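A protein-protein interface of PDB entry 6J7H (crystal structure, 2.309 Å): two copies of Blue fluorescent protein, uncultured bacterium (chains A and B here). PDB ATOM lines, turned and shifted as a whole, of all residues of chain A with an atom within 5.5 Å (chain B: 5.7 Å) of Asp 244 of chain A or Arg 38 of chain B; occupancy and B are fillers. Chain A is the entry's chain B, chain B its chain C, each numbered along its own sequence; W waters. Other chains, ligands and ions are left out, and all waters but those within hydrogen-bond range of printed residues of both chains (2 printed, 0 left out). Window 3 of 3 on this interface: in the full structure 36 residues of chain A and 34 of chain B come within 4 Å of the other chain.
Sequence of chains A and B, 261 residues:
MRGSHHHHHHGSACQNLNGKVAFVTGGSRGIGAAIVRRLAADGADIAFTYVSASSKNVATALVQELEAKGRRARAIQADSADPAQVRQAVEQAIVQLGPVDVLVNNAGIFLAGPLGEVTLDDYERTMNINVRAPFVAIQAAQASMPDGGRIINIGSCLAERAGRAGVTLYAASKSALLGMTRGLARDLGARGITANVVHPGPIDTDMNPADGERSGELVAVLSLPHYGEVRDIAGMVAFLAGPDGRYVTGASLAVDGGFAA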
ATOM      1  N   PHE A 239      -2.515 -22.100  38.444  1.00  0.00           N
ATOM      2  CA  PHE A 239      -2.135 -22.432  37.078  1.00  0.00           C
ATOM      3  C   PHE A 239      -1.541 -21.219  36.374  1.00  0.00           C
ATOM      4  O   PHE A 239      -0.506 -21.314  35.702  1.00  0.00           O
ATOM      5  CB  PHE A 239      -3.363 -22.945  36.313  1.00  0.00           C
ATOM      6  CG  PHE A 239      -3.148 -23.048  34.833  1.00  0.00           C
ATOM      7  CD1 PHE A 239      -2.566 -24.176  34.284  1.00  0.00           C
ATOM      8  CD2 PHE A 239      -3.488 -22.000  33.998  1.00  0.00           C
ATOM      9  CE1 PHE A 239      -2.353 -24.268  32.922  1.00  0.00           C
ATOM     10  CE2 PHE A 239      -3.274 -22.083  32.635  1.00  0.00           C
ATOM     11  CZ  PHE A 239      -2.701 -23.221  32.098  1.00  0.00           C
ATOM     12  N   GLY A 242       1.996 -20.299  37.595  1.00  0.00           N
ATOM     13  CA  GLY A 242       3.040 -21.273  37.384  1.00  0.00           C
ATOM     14  C   GLY A 242       3.598 -21.334  35.976  1.00  0.00           C
ATOM     15  O   GLY A 242       3.329 -20.485  35.121  1.00  0.00           O
ATOM     16  N   PRO A 243       4.448 -22.336  35.744  1.00  0.00           N
ATOM     17  CA  PRO A 243       5.061 -22.530  34.417  1.00  0.00           C
ATOM     18  C   PRO A 243       4.067 -22.754  33.287  1.00  0.00           C
ATOM     19  O   PRO A 243       4.366 -22.429  32.129  1.00  0.00           O
ATOM     20  CB  PRO A 243       5.949 -23.766  34.628  1.00  0.00           C
ATOM     21  CG  PRO A 243       5.310 -24.487  35.772  1.00  0.00           C
ATOM     22  CD  PRO A 243       4.795 -23.415  36.682  1.00  0.00           C
ATOM     23  N   ASP A 244       2.925 -23.371  33.581  1.00  0.00           N
ATOM     24  CA  ASP A 244       1.940 -23.661  32.553  1.00  0.00           C
ATOM     25  C   ASP A 244       1.182 -22.414  32.090  1.00  0.00           C
ATOM     26  O   ASP A 244       0.546 -22.456  31.037  1.00  0.00           O
ATOM     27  CB  ASP A 244       0.963 -24.726  33.060  1.00  0.00           C
ATOM     28  CG  ASP A 244       1.585 -26.123  33.120  1.00  0.00           C
ATOM     29  OD1 ASP A 244       2.530 -26.403  32.351  1.00  0.00           O
ATOM     30  OD2 ASP A 244       1.116 -26.948  33.938  1.00  0.00           O
ATOM     31  N   GLY A 245       1.243 -21.311  32.837  1.00  0.00           N
ATOM     32  CA  GLY A 245       0.593 -20.057  32.499  1.00  0.00           C
ATOM     33  C   GLY A 245       1.452 -19.075  31.732  1.00  0.00           C
ATOM     34  O   GLY A 245       1.074 -17.908  31.573  1.00  0.00           O
ATOM     35  N   ARG A 246       2.616 -19.527  31.271  1.00  0.00           N
ATOM     36  CA  ARG A 246       3.641 -18.651  30.716  1.00  0.00           C
ATOM     37  C   ARG A 246       3.190 -17.948  29.434  1.00  0.00           C
ATOM     38  O   ARG A 246       3.596 -16.806  29.173  1.00  0.00           O
ATOM     39  CB  ARG A 246       4.861 -19.536  30.436  1.00  0.00           C
ATOM     40  CG  ARG A 246       6.217 -18.904  30.330  1.00  0.00           C
ATOM     41  CD  ARG A 246       7.271 -20.015  30.193  1.00  0.00           C
ATOM     42  NE  ARG A 246       7.262 -20.673  28.880  1.00  0.00           N
ATOM     43  CZ  ARG A 246       6.626 -21.810  28.594  1.00  0.00           C
ATOM     44  NH1 ARG A 246       5.923 -22.436  29.529  1.00  0.00           N
ATOM     45  NH2 ARG A 246       6.698 -22.332  27.373  1.00  0.00           N
ATOM     46  N   TYR A 247       2.337 -18.595  28.640  1.00  0.00           N
ATOM     47  CA  TYR A 247       1.899 -18.057  27.359  1.00  0.00           C
ATOM     48  C   TYR A 247       0.442 -17.586  27.371  1.00  0.00           C
ATOM     49  O   TYR A 247      -0.117 -17.304  26.301  1.00  0.00           O
ATOM     50  CB  TYR A 247       2.141 -19.093  26.253  1.00  0.00           C
ATOM     51  CG  TYR A 247       2.299 -18.499  24.869  1.00  0.00           C
ATOM     52  CD1 TYR A 247       3.330 -17.608  24.579  1.00  0.00           C
ATOM     53  CD2 TYR A 247       1.403 -18.817  23.856  1.00  0.00           C
ATOM     54  CE1 TYR A 247       3.470 -17.064  23.310  1.00  0.00           C
ATOM     55  CE2 TYR A 247       1.530 -18.282  22.596  1.00  0.00           C
ATOM     56  CZ  TYR A 247       2.561 -17.407  22.319  1.00  0.00           C
ATOM     57  OH  TYR A 247       2.663 -16.872  21.041  1.00  0.00           O
ATOM     58  N   VAL A 248      -0.194 -17.544  28.544  1.00  0.00           N
ATOM     59  CA  VAL A 248      -1.560 -17.042  28.720  1.00  0.00           C
ATOM     60  C   VAL A 248      -1.481 -15.604  29.222  1.00  0.00           C
ATOM     61  O   VAL A 248      -1.036 -15.359  30.351  1.00  0.00           O
ATOM     62  CB  VAL A 248      -2.367 -17.909  29.700  1.00  0.00           C
ATOM     63  CG1 VAL A 248      -3.780 -17.349  29.864  1.00  0.00           C
ATOM     64  CG2 VAL A 248      -2.409 -19.372  29.243  1.00  0.00           C
ATOM     65  N   ALA B  33       0.544 -34.761  19.835  1.00  0.00           N
ATOM     66  CA  ALA B  33       1.531 -35.616  20.479  1.00  0.00           C
ATOM     67  C   ALA B  33       1.913 -35.085  21.854  1.00  0.00           C
ATOM     68  O   ALA B  33       2.063 -35.865  22.805  1.00  0.00           O
ATOM     69  CB  ALA B  33       2.771 -35.745  19.589  1.00  0.00           C
ATOM     70  N   ALA B  34       2.047 -33.763  21.990  1.00  0.00           N
ATOM     71  CA  ALA B  34       2.371 -33.190  23.290  1.00  0.00           C
ATOM     72  C   ALA B  34       1.245 -33.417  24.281  1.00  0.00           C
ATOM     73  O   ALA B  34       1.495 -33.685  25.465  1.00  0.00           O
ATOM     74  CB  ALA B  34       2.665 -31.692  23.154  1.00  0.00           C
ATOM     75  N   ILE B  35       0.002 -33.375  23.798  1.00  0.00           N
ATOM     76  CA  ILE B  35      -1.148 -33.578  24.666  1.00  0.00           C
ATOM     77  C   ILE B  35      -1.177 -35.008  25.180  1.00  0.00           C
ATOM     78  O   ILE B  35      -1.327 -35.247  26.383  1.00  0.00           O
ATOM     79  CB  ILE B  35      -2.448 -33.228  23.915  1.00  0.00           C
ATOM     80  CG1 ILE B  35      -2.602 -31.711  23.751  1.00  0.00           C
ATOM     81  CG2 ILE B  35      -3.672 -33.889  24.578  1.00  0.00           C
ATOM     82  CD1 ILE B  35      -3.755 -31.320  22.820  1.00  0.00           C
ATOM     83  N   VAL B  36      -0.981 -35.979  24.284  1.00  0.00           N
ATOM     84  CA  VAL B  36      -1.028 -37.371  24.711  1.00  0.00           C
ATOM     85  C   VAL B  36       0.126 -37.685  25.662  1.00  0.00           C
ATOM     86  O   VAL B  36      -0.053 -38.416  26.642  1.00  0.00           O
ATOM     87  CB  VAL B  36      -1.043 -38.314  23.490  1.00  0.00           C
ATOM     88  CG1 VAL B  36      -2.208 -38.010  22.550  1.00  0.00           C
ATOM     89  CG2 VAL B  36       0.261 -38.293  22.769  1.00  0.00           C
ATOM     90  N   ARG B  37       1.311 -37.103  25.425  1.00  0.00           N
ATOM     91  CA  ARG B  37       2.436 -37.340  26.331  1.00  0.00           C
ATOM     92  C   ARG B  37       2.166 -36.733  27.694  1.00  0.00           C
ATOM     93  O   ARG B  37       2.452 -37.350  28.725  1.00  0.00           O
ATOM     94  CB  ARG B  37       3.737 -36.770  25.753  1.00  0.00           C
ATOM     95  CG  ARG B  37       4.335 -37.577  24.601  1.00  0.00           C
ATOM     96  CD  ARG B  37       5.709 -37.043  24.176  1.00  0.00           C
ATOM     97  NE  ARG B  37       6.403 -37.977  23.287  1.00  0.00           N
ATOM     98  CZ  ARG B  37       6.475 -37.853  21.966  1.00  0.00           C
ATOM     99  NH1 ARG B  37       5.904 -36.824  21.364  1.00  0.00           N
ATOM    100  NH2 ARG B  37       7.118 -38.765  21.246  1.00  0.00           N
ATOM    101  N   ARG B  38       1.612 -35.524  27.721  1.00  0.00           N
ATOM    102  CA  ARG B  38       1.312 -34.891  28.996  1.00  0.00           C
ATOM    103  C   ARG B  38       0.235 -35.663  29.749  1.00  0.00           C
ATOM    104  O   ARG B  38       0.379 -35.937  30.944  1.00  0.00           O
ATOM    105  CB  ARG B  38       0.887 -33.441  28.764  1.00  0.00           C
ATOM    106  CG  ARG B  38       0.537 -32.702  30.031  1.00  0.00           C
ATOM    107  CD  ARG B  38       1.753 -32.566  30.911  1.00  0.00           C
ATOM    108  NE  ARG B  38       1.407 -31.959  32.188  1.00  0.00           N
ATOM    109  CZ  ARG B  38       1.506 -30.659  32.449  1.00  0.00           C
ATOM    110  NH1 ARG B  38       1.165 -30.199  33.646  1.00  0.00           N
ATOM    111  NH2 ARG B  38       1.959 -29.823  31.519  1.00  0.00           N
ATOM    112  N   LEU B  39      -0.836 -36.064  29.058  1.00  0.00           N
ATOM    113  CA  LEU B  39      -1.885 -36.809  29.745  1.00  0.00           C
ATOM    114  C   LEU B  39      -1.367 -38.149  30.266  1.00  0.00           C
ATOM    115  O   LEU B  39      -1.737 -38.577  31.368  1.00  0.00           O
ATOM    116  CB  LEU B  39      -3.076 -37.014  28.808  1.00  0.00           C
ATOM    117  CG  LEU B  39      -3.840 -35.745  28.410  1.00  0.00           C
ATOM    118  CD1 LEU B  39      -5.013 -36.077  27.506  1.00  0.00           C
ATOM    119  CD2 LEU B  39      -4.320 -35.005  29.649  1.00  0.00           C
ATOM    120  N   ALA B  40      -0.480 -38.805  29.506  1.00  0.00           N
ATOM    121  CA  ALA B  40       0.101 -40.064  29.965  1.00  0.00           C
ATOM    122  C   ALA B  40       1.015 -39.847  31.167  1.00  0.00           C
ATOM    123  O   ALA B  40       1.010 -40.649  32.105  1.00  0.00           O
ATOM    124  CB  ALA B  40       0.854 -40.750  28.820  1.00  0.00           C
ATOM    125  N   ALA B  41       1.770 -38.743  31.181  1.00  0.00           N
ATOM    126  CA  ALA B  41       2.635 -38.458  32.321  1.00  0.00           C
ATOM    127  C   ALA B  41       1.827 -38.185  33.581  1.00  0.00           C
ATOM    128  O   ALA B  41       2.343 -38.352  34.689  1.00  0.00           O
ATOM    129  CB  ALA B  41       3.560 -37.276  32.019  1.00  0.00           C
ATOM    130  N   ASP B  42       0.578 -37.762  33.441  1.00  0.00           N
ATOM    131  CA  ASP B  42      -0.304 -37.609  34.587  1.00  0.00           C
ATOM    132  C   ASP B  42      -1.022 -38.909  34.929  1.00  0.00           C
ATOM    133  O   ASP B  42      -1.861 -38.921  35.834  1.00  0.00           O
ATOM    134  CB  ASP B  42      -1.310 -36.490  34.324  1.00  0.00           C
ATOM    135  CG  ASP B  42      -0.645 -35.121  34.258  1.00  0.00           C
ATOM    136  OD1 ASP B  42       0.532 -35.009  34.666  1.00  0.00           O
ATOM    137  OD2 ASP B  42      -1.295 -34.156  33.794  1.00  0.00           O
ATOM    138  N   GLY B  43      -0.704 -39.999  34.224  1.00  0.00           N
ATOM    139  CA  GLY B  43      -1.179 -41.330  34.550  1.00  0.00           C
ATOM    140  C   GLY B  43      -2.362 -41.852  33.761  1.00  0.00           C
ATOM    141  O   GLY B  43      -2.799 -42.977  34.022  1.00  0.00           O
ATOM    142  N   ARG B 231       4.024 -27.418  24.499  1.00  0.00           N
ATOM    143  CA  ARG B 231       3.806 -27.658  25.923  1.00  0.00           C
ATOM    144  C   ARG B 231       2.822 -26.668  26.542  1.00  0.00           C
ATOM    145  O   ARG B 231       2.081 -27.030  27.460  1.00  0.00           O
ATOM    146  CB  ARG B 231       5.136 -27.606  26.673  1.00  0.00           C
ATOM    147  CG  ARG B 231       5.910 -26.319  26.412  1.00  0.00           C
ATOM    148  CD  ARG B 231       7.023 -26.088  27.418  1.00  0.00           C
ATOM    149  NE  ARG B 231       6.472 -25.618  28.688  1.00  0.00           N
ATOM    150  CZ  ARG B 231       7.110 -25.658  29.855  1.00  0.00           C
ATOM    151  NH1 ARG B 231       8.332 -26.173  29.925  1.00  0.00           N
ATOM    152  NH2 ARG B 231       6.518 -25.182  30.953  1.00  0.00           N
ATOM    153  N   ASP B 232       2.760 -25.435  26.030  1.00  0.00           N
ATOM    154  CA  ASP B 232       1.785 -24.479  26.544  1.00  0.00           C
ATOM    155  C   ASP B 232       0.362 -24.958  26.288  1.00  0.00           C
ATOM    156  O   ASP B 232      -0.518 -24.794  27.141  1.00  0.00           O
ATOM    157  CB  ASP B 232       2.018 -23.111  25.912  1.00  0.00           C
ATOM    158  CG  ASP B 232       3.395 -22.557  26.211  1.00  0.00           C
ATOM    159  OD1 ASP B 232       3.789 -22.532  27.398  1.00  0.00           O
ATOM    160  OD2 ASP B 232       4.100 -22.174  25.250  1.00  0.00           O
ATOM    161  N   ALA B 234      -0.452 -28.199  25.787  1.00  0.00           N
ATOM    162  CA  ALA B 234      -0.603 -29.416  26.569  1.00  0.00           C
ATOM    163  C   ALA B 234      -0.815 -29.110  28.045  1.00  0.00           C
ATOM    164  O   ALA B 234      -1.533 -29.849  28.730  1.00  0.00           O
ATOM    165  CB  ALA B 234       0.623 -30.306  26.375  1.00  0.00           C
ATOM    166  N   GLY B 235      -0.205 -28.034  28.553  1.00  0.00           N
ATOM    167  CA  GLY B 235      -0.406 -27.672  29.953  1.00  0.00           C
ATOM    168  C   GLY B 235      -1.798 -27.134  30.240  1.00  0.00           C
ATOM    169  O   GLY B 235      -2.375 -27.407  31.299  1.00  0.00           O
ATOM    170  N   MET B 236      -2.363 -26.363  29.305  1.00  0.00           N
ATOM    171  CA  MET B 236      -3.744 -25.925  29.474  1.00  0.00           C
ATOM    172  C   MET B 236      -4.702 -27.110  29.426  1.00  0.00           C
ATOM    173  O   MET B 236      -5.608 -27.223  30.260  1.00  0.00           O
ATOM    174  CB  MET B 236      -4.105 -24.900  28.396  1.00  0.00           C
ATOM    175  CG  MET B 236      -5.562 -24.461  28.407  1.00  0.00           C
ATOM    176  SD  MET B 236      -6.076 -23.683  29.959  1.00  0.00           S
ATOM    177  CE  MET B 236      -5.388 -22.032  29.799  1.00  0.00           C
ATOM    178  N   ALA B 238      -3.963 -30.234  30.126  1.00  0.00           N
ATOM    179  CA  ALA B 238      -3.800 -30.998  31.356  1.00  0.00           C
ATOM    180  C   ALA B 238      -4.533 -30.326  32.514  1.00  0.00           C
ATOM    181  O   ALA B 238      -5.096 -31.006  33.377  1.00  0.00           O
ATOM    182  CB  ALA B 238      -2.318 -31.175  31.677  1.00  0.00           C
HETATM  183  O   HOH W   1       1.355 -21.208  28.622  1.00  0.00           O
HETATM  184  O   HOH W   2       6.019 -19.977  25.516  1.00  0.00           O
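Water W1 lies within hydrogen-bond range of N of Tyr 247 of chain A (2.8 Å), O of Asp 244 of chain A (2.8 Å), OD1 of Asp 232 of chain B (3.0 Å) and N of Arg 246 of chain A (3.4 Å). Water W2 lies within hydrogen-bond range of the side-chain carboxylate of Asp 232 of chain B and the guanidinium group of Arg 246 of chain A.
Printed residues of chain B within 4 Å of Pro 243 of chain A: Arg 231. Ala 34 of chain B touches none of the printed residues of chain A. Of chain A, only Asp 244 comes within 4 Å of Arg 38 of chain B. Of the printed residues of chain A, Gly 235 of chain B touches Phe 239 (3.5 Å) and Asp 244 (3.998 Å). The nearest printed residue of chain A that does not touch Arg 38 of chain B is Phe 239 of chain A (6.9 Å). The nearest printed residue of chain B that does not touch Arg 246 of chain A is Gly 235 of chain B (8.2 Å).
Gly 235 of chain B touches Phe 239 of chain A (O to CE1, 3.5 Å). Phe 239 of chain A touches Met 236 of chain B (CE2 to CE, 3.5 Å). Pro 243 of chain A touches Arg 231 of chain B. Asp 244 of chain A touches Gly 235 of chain B (OD1 to CA, 3.998 Å). CG of Asp 232 of chain B touches CB of Tyr 247 of chain A, at 3.7 Å.
No position is printed for both chains. Of the 8 pairs that touch across the chains among the printed residues, none has its exchanged pair printed and touching as well.
Hydrophobic or aromatic side chains of chain B within 4 Å of the printed part of chain A: Met 236. Of the 8 printed residues of chain A, 5 touch a printed residue of chain B. Printed residues of chain A that touch a printed residue of chain B: Phe 239, Pro 243, Asp 244, Arg 246 and Tyr 247. Hydrophobic or aromatic side chains of chain A that line the printed part of chain B: Phe 239, Pro 243 and Tyr 247. Along chain A the printed residues that touch a printed residue of chain B span positions 239 to 247. Among the printed residues, 8 pairs touch across the chains. Among the printed residues, Asp or Glu carboxylates within 4 Å of a Lys or Arg side-chain nitrogen of the other chain: Asp 244 of chain A with Arg 38 of chain B and Arg 246 of chain A with Asp 232 of chain B.
NH1 of Arg 38 of chain B is in salt-bridge range of OD2 of Asp 244 of chain A (3.3 Å). The guanidinium group (NH2) of Arg 246 of chain A is in salt-bridge range of the side-chain carboxylate (OD1) of Asp 232 of chain B (2.9 Å). NH1 of Arg 246 of chain A sits close to NH2 of Arg 231 of chain B (3.1 Å).
The backbone NH (N) of Gly 245 of chain A is in hydrogen-bond range of the backbone carbonyl oxygen (O) of Phe 239 of chain A. O of Pro 243 of chain A is in hydrogen-bond range of NH1 of Arg 246 of chain A, 3.0 Å away. The side-chain carboxylate of Asp 42 of chain B lies within salt-bridge range of the guanidinium group of Arg 38 of chain B (3.8 Å).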
